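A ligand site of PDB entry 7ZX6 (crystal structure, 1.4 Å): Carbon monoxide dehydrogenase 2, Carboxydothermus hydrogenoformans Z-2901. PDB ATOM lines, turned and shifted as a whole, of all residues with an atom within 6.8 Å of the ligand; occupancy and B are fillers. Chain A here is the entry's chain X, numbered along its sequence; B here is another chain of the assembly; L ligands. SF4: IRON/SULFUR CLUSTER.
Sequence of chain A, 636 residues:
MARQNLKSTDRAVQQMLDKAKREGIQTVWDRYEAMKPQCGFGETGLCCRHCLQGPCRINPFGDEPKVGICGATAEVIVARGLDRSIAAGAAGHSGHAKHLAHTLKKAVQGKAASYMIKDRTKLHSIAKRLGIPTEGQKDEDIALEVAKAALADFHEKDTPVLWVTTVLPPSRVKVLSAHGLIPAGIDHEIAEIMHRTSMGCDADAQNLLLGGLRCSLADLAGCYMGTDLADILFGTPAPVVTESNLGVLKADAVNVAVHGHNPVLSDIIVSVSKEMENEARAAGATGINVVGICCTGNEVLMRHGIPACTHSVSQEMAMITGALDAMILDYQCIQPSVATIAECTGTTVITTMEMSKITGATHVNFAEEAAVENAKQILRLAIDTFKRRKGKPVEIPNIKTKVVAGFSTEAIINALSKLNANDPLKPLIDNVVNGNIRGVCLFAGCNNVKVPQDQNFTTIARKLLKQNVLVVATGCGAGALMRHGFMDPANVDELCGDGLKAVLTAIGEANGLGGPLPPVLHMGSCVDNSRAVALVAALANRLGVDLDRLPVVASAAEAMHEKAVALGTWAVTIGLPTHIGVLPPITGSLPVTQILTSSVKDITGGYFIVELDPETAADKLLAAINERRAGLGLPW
N of Gly 54 lies close to S4 of the ligand, at 3.7 Å.
The guanidinium group (NH2) of Arg 80 lies close to a sulfur (S1) of the ligand (3.7 Å).
FE1 of the ligand is bound by SG of Cys 56, at 2.3 Å.
N of Cys 51 sits close to S4 of the ligand.
The side-chain sulfur (SG) of Cys 48 is bound to an iron atom (FE3) of the ligand.
A sulfur (S3) of the ligand lies close to the side-chain amide oxygen (OE1) of Gln 53 (3.8 Å).
The backbone NH (N) of Cys 70 lies close to a sulfur (S3) of the ligand (3.5 Å).
FE4 of the ligand is bound by SG of Cys 70.
SG of Cys 51 is bound to FE2 of the ligand (2.3 Å).
The backbone carbonyl oxygen (O) of Gln 53 is in hydrogen-bond range of the side-chain amide nitrogen (NE2) of Gln 38 of chain B (2.9 Å).
The backbone carbonyl oxygen of Cys 56 is in hydrogen-bond range of the backbone NH of Cys 48.
The side-chain sulfur (SG) of Cys 48 sits close to the guanidinium group (NH2) of Arg 80 (3.4 Å).
The side-chain sulfur (SG) of Cys 51 sits close to the backbone NH (N) of Gln 53.
SG of Cys 70 sits close to N of Ala 72 (3.6 Å).
A ring nitrogen (ND1) of His 50 sits at hydrogen-bond distance from the backbone carbonyl oxygen of Thr 197, at 2.8 Å.
The side-chain sulfur (SG) of Cys 47 lies close to the backbone carbonyl oxygen (O) of Cys 56.
The side-chain sulfur (SG) of Cys 56 sits close to the backbone NH (N) of Ile 69, 3.4 Å away.
His 50 touches the ligand.
Gly 68 touches the ligand.
CB of Ile 69 touches S3 of the ligand (3.8 Å).
Ala 72 touches the ligand (CB to S2, 3.99 Å).
Met 199 touches the ligand (CG to S1, 3.6 Å).
Hydrophobic or aromatic side chains that line the ligand: Ile 69, Ala 72 and Met 199.
The nearest printed residue that does not touch the ligand is Arg 49 (4.2 Å).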
ATOM      1  N   CYS A  47      15.953 -15.390  -7.074  1.00  0.00           N
ATOM      2  CA  CYS A  47      16.440 -15.512  -5.705  1.00  0.00           C
ATOM      3  C   CYS A  47      15.297 -15.134  -4.763  1.00  0.00           C
ATOM      4  O   CYS A  47      14.555 -14.183  -5.040  1.00  0.00           O
ATOM      5  CB  CYS A  47      17.666 -14.635  -5.463  1.00  0.00           C
ATOM      6  SG  CYS A  47      18.204 -14.708  -3.699  1.00  0.00           S
ATOM      7  N   CYS A  48      15.186 -15.853  -3.643  1.00  0.00           N
ATOM      8  CA  CYS A  48      14.126 -15.559  -2.676  1.00  0.00           C
ATOM      9  C   CYS A  48      14.719 -15.663  -1.283  1.00  0.00           C
ATOM     10  O   CYS A  48      15.422 -16.625  -0.964  1.00  0.00           O
ATOM     11  CB  CYS A  48      12.969 -16.559  -2.812  1.00  0.00           C
ATOM     12  SG  CYS A  48      11.660 -16.304  -1.610  1.00  0.00           S
ATOM     13  N   ARG A  49      14.423 -14.668  -0.446  1.00  0.00           N
ATOM     14  CA  ARG A  49      14.841 -14.634   0.950  1.00  0.00           C
ATOM     15  C   ARG A  49      13.632 -14.390   1.835  1.00  0.00           C
ATOM     16  O   ARG A  49      13.749 -13.758   2.887  1.00  0.00           O
ATOM     17  CB  ARG A  49      15.916 -13.563   1.176  1.00  0.00           C
ATOM     18  CG  ARG A  49      17.212 -13.823   0.378  1.00  0.00           C
ATOM     19  CD  ARG A  49      18.183 -12.632   0.413  1.00  0.00           C
ATOM     20  NE  ARG A  49      18.488 -12.298   1.790  1.00  0.00           N
ATOM     21  CZ  ARG A  49      18.926 -11.108   2.182  1.00  0.00           C
ATOM     22  NH1 ARG A  49      19.162 -10.150   1.301  1.00  0.00           N
ATOM     23  NH2 ARG A  49      19.165 -10.897   3.482  1.00  0.00           N
ATOM     24  N   HIS A  50      12.460 -14.869   1.416  1.00  0.00           N
ATOM     25  CA  HIS A  50      11.238 -14.570   2.156  1.00  0.00           C
ATOM     26  C   HIS A  50      11.044 -15.439   3.379  1.00  0.00           C
ATOM     27  O   HIS A  50      10.037 -15.267   4.076  1.00  0.00           O
ATOM     28  CB  HIS A  50       9.986 -14.615   1.268  1.00  0.00           C
ATOM     29  CG  HIS A  50       9.959 -13.547   0.209  1.00  0.00           C
ATOM     30  ND1 HIS A  50       8.819 -13.218  -0.487  1.00  0.00           N
ATOM     31  CD2 HIS A  50      10.931 -12.736  -0.269  1.00  0.00           C
ATOM     32  CE1 HIS A  50       9.079 -12.251  -1.352  1.00  0.00           C
ATOM     33  NE2 HIS A  50      10.359 -11.927  -1.235  1.00  0.00           N
ATOM     34  N   CYS A  51      11.943 -16.354   3.659  1.00  0.00           N
ATOM     35  CA  CYS A  51      11.906 -17.026   4.956  1.00  0.00           C
ATOM     36  C   CYS A  51      13.312 -17.463   5.343  1.00  0.00           C
ATOM     37  O   CYS A  51      14.249 -17.396   4.551  1.00  0.00           O
ATOM     38  CB  CYS A  51      10.910 -18.203   4.995  1.00  0.00           C
ATOM     39  SG  CYS A  51      11.519 -19.777   4.258  1.00  0.00           S
ATOM     40  N   LEU A  52      13.453 -17.950   6.567  1.00  0.00           N
ATOM     41  CA  LEU A  52      14.762 -18.331   7.088  1.00  0.00           C
ATOM     42  C   LEU A  52      15.216 -19.711   6.664  1.00  0.00           C
ATOM     43  O   LEU A  52      16.297 -20.154   7.103  1.00  0.00           O
ATOM     44  CB  LEU A  52      14.783 -18.225   8.613  1.00  0.00           C
ATOM     45  CG  LEU A  52      14.393 -16.860   9.163  1.00  0.00           C
ATOM     46  CD1 LEU A  52      14.413 -16.905  10.693  1.00  0.00           C
ATOM     47  CD2 LEU A  52      15.366 -15.806   8.665  1.00  0.00           C
ATOM     48  N   GLN A  53      14.458 -20.408   5.820  1.00  0.00           N
ATOM     49  CA  GLN A  53      15.009 -21.564   5.123  1.00  0.00           C
ATOM     50  C   GLN A  53      15.889 -21.171   3.952  1.00  0.00           C
ATOM     51  O   GLN A  53      16.682 -21.996   3.497  1.00  0.00           O
ATOM     52  CB  GLN A  53      13.884 -22.477   4.634  1.00  0.00           C
ATOM     53  CG  GLN A  53      13.156 -23.123   5.789  1.00  0.00           C
ATOM     54  CD  GLN A  53      11.975 -23.991   5.398  1.00  0.00           C
ATOM     55  OE1 GLN A  53      11.274 -23.710   4.396  1.00  0.00           O
ATOM     56  NE2 GLN A  53      11.724 -25.020   6.164  1.00  0.00           N
ATOM     57  N   GLY A  54      15.749 -19.924   3.456  1.00  0.00           N
ATOM     58  CA  GLY A  54      16.536 -19.452   2.336  1.00  0.00           C
ATOM     59  C   GLY A  54      17.924 -19.032   2.798  1.00  0.00           C
ATOM     60  O   GLY A  54      18.339 -19.273   3.944  1.00  0.00           O
ATOM     61  N   PRO A  55      18.672 -18.377   1.924  1.00  0.00           N
ATOM     62  CA  PRO A  55      18.270 -17.956   0.573  1.00  0.00           C
ATOM     63  C   PRO A  55      18.058 -19.126  -0.357  1.00  0.00           C
ATOM     64  O   PRO A  55      18.800 -20.121  -0.352  1.00  0.00           O
ATOM     65  CB  PRO A  55      19.432 -17.049   0.120  1.00  0.00           C
ATOM     66  CG  PRO A  55      20.594 -17.438   1.052  1.00  0.00           C
ATOM     67  CD  PRO A  55      20.065 -18.040   2.273  1.00  0.00           C
ATOM     68  N   CYS A  56      17.031 -19.002  -1.176  1.00  0.00           N
ATOM     69  CA  CYS A  56      16.784 -19.941  -2.255  1.00  0.00           C
ATOM     70  C   CYS A  56      17.113 -19.279  -3.576  1.00  0.00           C
ATOM     71  O   CYS A  56      16.859 -18.094  -3.775  1.00  0.00           O
ATOM     72  CB  CYS A  56      15.321 -20.367  -2.251  1.00  0.00           C
ATOM     73  SG  CYS A  56      14.914 -21.493  -0.875  1.00  0.00           S
ATOM     74  N   ARG A  57      17.688 -20.054  -4.466  1.00  0.00           N
ATOM     75  CA  ARG A  57      17.962 -19.557  -5.800  1.00  0.00           C
ATOM     76  C   ARG A  57      17.533 -20.633  -6.766  1.00  0.00           C
ATOM     77  O   ARG A  57      17.252 -21.782  -6.393  1.00  0.00           O
ATOM     78  CB  ARG A  57      19.436 -19.230  -5.973  1.00  0.00           C
ATOM     79  CG  ARG A  57      20.264 -20.473  -6.154  1.00  0.00           C
ATOM     80  CD  ARG A  57      21.714 -20.251  -5.736  1.00  0.00           C
ATOM     81  NE  ARG A  57      22.442 -21.505  -5.847  1.00  0.00           N
ATOM     82  CZ  ARG A  57      22.462 -22.440  -4.910  1.00  0.00           C
ATOM     83  NH1 ARG A  57      23.132 -23.566  -5.140  1.00  0.00           N
ATOM     84  NH2 ARG A  57      21.827 -22.282  -3.722  1.00  0.00           N
ATOM     85  N   VAL A  67      13.848 -25.266  -8.071  1.00  0.00           N
ATOM     86  CA  VAL A  67      12.628 -24.876  -7.368  1.00  0.00           C
ATOM     87  C   VAL A  67      13.054 -24.486  -5.953  1.00  0.00           C
ATOM     88  O   VAL A  67      14.074 -24.975  -5.442  1.00  0.00           O
ATOM     89  CB  VAL A  67      11.633 -26.065  -7.374  1.00  0.00           C
ATOM     90  CG1 VAL A  67      12.255 -27.318  -6.735  1.00  0.00           C
ATOM     91  CG2 VAL A  67      10.313 -25.731  -6.747  1.00  0.00           C
ATOM     92  N   GLY A  68      12.314 -23.542  -5.355  1.00  0.00           N
ATOM     93  CA  GLY A  68      12.590 -23.133  -3.977  1.00  0.00           C
ATOM     94  C   GLY A  68      12.346 -24.261  -2.987  1.00  0.00           C
ATOM     95  O   GLY A  68      11.677 -25.246  -3.306  1.00  0.00           O
ATOM     96  N   ILE A  69      12.893 -24.092  -1.774  1.00  0.00           N
ATOM     97  CA  ILE A  69      12.800 -25.158  -0.775  1.00  0.00           C
ATOM     98  C   ILE A  69      11.344 -25.497  -0.451  1.00  0.00           C
ATOM     99  O   ILE A  69      10.987 -26.669  -0.293  1.00  0.00           O
ATOM    100  CB  ILE A  69      13.627 -24.807   0.473  1.00  0.00           C
ATOM    101  CG1 ILE A  69      15.101 -24.897   0.119  1.00  0.00           C
ATOM    102  CG2 ILE A  69      13.306 -25.728   1.639  1.00  0.00           C
ATOM    103  CD1 ILE A  69      16.040 -24.366   1.198  1.00  0.00           C
ATOM    104  N   CYS A  70      10.481 -24.478  -0.332  1.00  0.00           N
ATOM    105  CA  CYS A  70       9.086 -24.701   0.006  1.00  0.00           C
ATOM    106  C   CYS A  70       8.268 -25.175  -1.193  1.00  0.00           C
ATOM    107  O   CYS A  70       7.064 -25.463  -1.050  1.00  0.00           O
ATOM    108  CB  CYS A  70       8.475 -23.415   0.575  1.00  0.00           C
ATOM    109  SG  CYS A  70       8.569 -22.092  -0.707  1.00  0.00           S
ATOM    110  N   GLY A  71       8.907 -25.289  -2.374  1.00  0.00           N
ATOM    111  CA  GLY A  71       8.223 -25.609  -3.616  1.00  0.00           C
ATOM    112  C   GLY A  71       7.915 -24.411  -4.495  1.00  0.00           C
ATOM    113  O   GLY A  71       7.313 -24.583  -5.565  1.00  0.00           O
ATOM    114  N   ALA A  72       8.318 -23.200  -4.100  1.00  0.00           N
ATOM    115  CA  ALA A  72       8.053 -22.028  -4.922  1.00  0.00           C
ATOM    116  C   ALA A  72       8.750 -22.140  -6.268  1.00  0.00           C
ATOM    117  O   ALA A  72       9.978 -22.330  -6.355  1.00  0.00           O
ATOM    118  CB  ALA A  72       8.518 -20.762  -4.207  1.00  0.00           C
ATOM    119  N   ILE A  77       8.478 -17.048  -7.504  1.00  0.00           N
ATOM    120  CA  ILE A  77       9.566 -16.266  -6.911  1.00  0.00           C
ATOM    121  C   ILE A  77       9.714 -14.932  -7.646  1.00  0.00           C
ATOM    122  O   ILE A  77       9.775 -13.857  -7.016  1.00  0.00           O
ATOM    123  CB  ILE A  77      10.875 -17.085  -6.914  1.00  0.00           C
ATOM    124  CG1 ILE A  77      10.812 -18.170  -5.842  1.00  0.00           C
ATOM    125  CG2 ILE A  77      12.075 -16.157  -6.719  1.00  0.00           C
ATOM    126  CD1 ILE A  77      11.958 -19.182  -6.001  1.00  0.00           C
ATOM    127  N   ARG A  80       6.657 -12.667  -6.870  1.00  0.00           N
ATOM    128  CA  ARG A  80       6.621 -12.156  -5.499  1.00  0.00           C
ATOM    129  C   ARG A  80       7.636 -11.037  -5.310  1.00  0.00           C
ATOM    130  O   ARG A  80       7.338 -10.030  -4.651  1.00  0.00           O
ATOM    131  CB  ARG A  80       6.918 -13.290  -4.500  1.00  0.00           C
ATOM    132  CG  ARG A  80       5.779 -14.336  -4.459  1.00  0.00           C
ATOM    133  CD  ARG A  80       5.876 -15.284  -3.251  1.00  0.00           C
ATOM    134  NE  ARG A  80       7.174 -15.934  -3.220  1.00  0.00           N
ATOM    135  CZ  ARG A  80       7.425 -17.004  -2.460  1.00  0.00           C
ATOM    136  NH1 ARG A  80       6.454 -17.562  -1.736  1.00  0.00           N
ATOM    137  NH2 ARG A  80       8.648 -17.552  -2.463  1.00  0.00           N
ATOM    138  N   THR A 197       2.798 -12.218  -0.570  1.00  0.00           N
ATOM    139  CA  THR A 197       4.111 -12.630  -1.040  1.00  0.00           C
ATOM    140  C   THR A 197       4.968 -13.270   0.053  1.00  0.00           C
ATOM    141  O   THR A 197       6.089 -13.710  -0.239  1.00  0.00           O
ATOM    142  CB  THR A 197       4.887 -11.435  -1.624  1.00  0.00           C
ATOM    143  OG1 THR A 197       4.996 -10.403  -0.625  1.00  0.00           O
ATOM    144  CG2 THR A 197       4.159 -10.847  -2.870  1.00  0.00           C
ATOM    145  N   SER A 198       4.495 -13.267   1.292  1.00  0.00           N
ATOM    146  CA  SER A 198       5.220 -13.968   2.359  1.00  0.00           C
ATOM    147  C   SER A 198       5.125 -15.490   2.178  1.00  0.00           C
ATOM    148  O   SER A 198       4.353 -16.004   1.339  1.00  0.00           O
ATOM    149  CB  SER A 198       4.739 -13.542   3.751  1.00  0.00           C
ATOM    150  OG  SER A 198       3.482 -14.102   4.041  1.00  0.00           O
ATOM    151  N   MET A 199       5.959 -16.243   2.919  1.00  0.00           N
ATOM    152  CA  MET A 199       6.087 -17.663   2.626  1.00  0.00           C
ATOM    153  C   MET A 199       4.749 -18.384   2.794  1.00  0.00           C
ATOM    154  O   MET A 199       3.989 -18.128   3.740  1.00  0.00           O
ATOM    155  CB  MET A 199       7.199 -18.291   3.509  1.00  0.00           C
ATOM    156  CG  MET A 199       7.400 -19.813   3.303  1.00  0.00           C
ATOM    157  SD  MET A 199       6.196 -20.758   4.291  1.00  0.00           S
ATOM    158  CE  MET A 199       6.414 -22.404   3.635  1.00  0.00           C
ATOM    159  N   GLY A 200       4.470 -19.294   1.867  1.00  0.00           N
ATOM    160  CA  GLY A 200       3.313 -20.167   1.975  1.00  0.00           C
ATOM    161  C   GLY A 200       1.973 -19.515   1.777  1.00  0.00           C
ATOM    162  O   GLY A 200       0.969 -19.994   2.334  1.00  0.00           O
ATOM    163  N   MET B  35      19.518 -27.381  -2.797  1.00  0.00           N
ATOM    164  CA  MET B  35      19.874 -25.978  -2.681  1.00  0.00           C
ATOM    165  C   MET B  35      21.257 -25.742  -2.083  1.00  0.00           C
ATOM    166  O   MET B  35      21.771 -24.616  -2.147  1.00  0.00           O
ATOM    167  CB  MET B  35      18.800 -25.268  -1.837  1.00  0.00           C
ATOM    168  CG  MET B  35      18.804 -23.748  -1.946  1.00  0.00           C
ATOM    169  SD  MET B  35      18.356 -23.206  -3.620  1.00  0.00           S
ATOM    170  CE  MET B  35      16.660 -23.702  -3.698  1.00  0.00           C
ATOM    171  N   GLN B  38      24.009 -23.002   0.193  1.00  0.00           N
ATOM    172  CA  GLN B  38      23.212 -21.811   0.006  1.00  0.00           C
ATOM    173  C   GLN B  38      24.099 -20.569   0.001  1.00  0.00           C
ATOM    174  O   GLN B  38      25.238 -20.571   0.491  1.00  0.00           O
ATOM    175  CB  GLN B  38      22.180 -21.708   1.110  1.00  0.00           C
ATOM    176  CG  GLN B  38      21.160 -22.836   1.048  1.00  0.00           C
ATOM    177  CD  GLN B  38      20.115 -22.737   2.124  1.00  0.00           C
ATOM    178  OE1 GLN B  38      20.340 -23.248   3.224  1.00  0.00           O
ATOM    179  NE2 GLN B  38      18.994 -22.085   1.829  1.00  0.00           N
ATOM    180  N   PRO B 336       3.862 -24.593  -1.318  1.00  0.00           N
ATOM    181  CA  PRO B 336       3.143 -24.741  -2.593  1.00  0.00           C
ATOM    182  C   PRO B 336       3.399 -26.061  -3.297  1.00  0.00           C
ATOM    183  O   PRO B 336       2.622 -26.421  -4.191  1.00  0.00           O
ATOM    184  CB  PRO B 336       3.591 -23.526  -3.416  1.00  0.00           C
ATOM    185  CG  PRO B 336       4.945 -23.109  -2.818  1.00  0.00           C
ATOM    186  CD  PRO B 336       4.759 -23.415  -1.328  1.00  0.00           C
ATOM    187  N   MET B 560      11.226 -19.974  11.130  1.00  0.00           N
ATOM    188  CA  MET B 560      11.238 -20.006   9.672  1.00  0.00           C
ATOM    189  C   MET B 560      10.582 -18.779   9.048  1.00  0.00           C
ATOM    190  O   MET B 560      11.189 -18.041   8.252  1.00  0.00           O
ATOM    191  CB  MET B 560      10.534 -21.271   9.186  1.00  0.00           C
ATOM    192  CG  MET B 560      10.448 -21.420   7.683  1.00  0.00           C
ATOM    193  SD  MET B 560       8.916 -20.790   6.913  1.00  0.00           S
ATOM    194  CE  MET B 560       7.687 -21.799   7.716  1.00  0.00           C
HETATM  195 FE1  SF4 L   1      12.972 -20.480  -0.070  1.00  0.00          FE
HETATM  196 FE2  SF4 L   1      11.606 -19.512   1.996  1.00  0.00          FE
HETATM  197 FE3  SF4 L   1      11.567 -18.301  -0.377  1.00  0.00          FE
HETATM  198 FE4  SF4 L   1      10.308 -20.637  -0.152  1.00  0.00          FE
HETATM  199  S1  SF4 L   1       9.826 -18.710   0.843  1.00  0.00           S
HETATM  200  S2  SF4 L   1      11.591 -20.026  -1.772  1.00  0.00           S
HETATM  201  S3  SF4 L   1      11.756 -21.652   1.282  1.00  0.00           S
HETATM  202  S4  SF4 L   1      13.293 -18.563   1.015  1.00  0.00           S
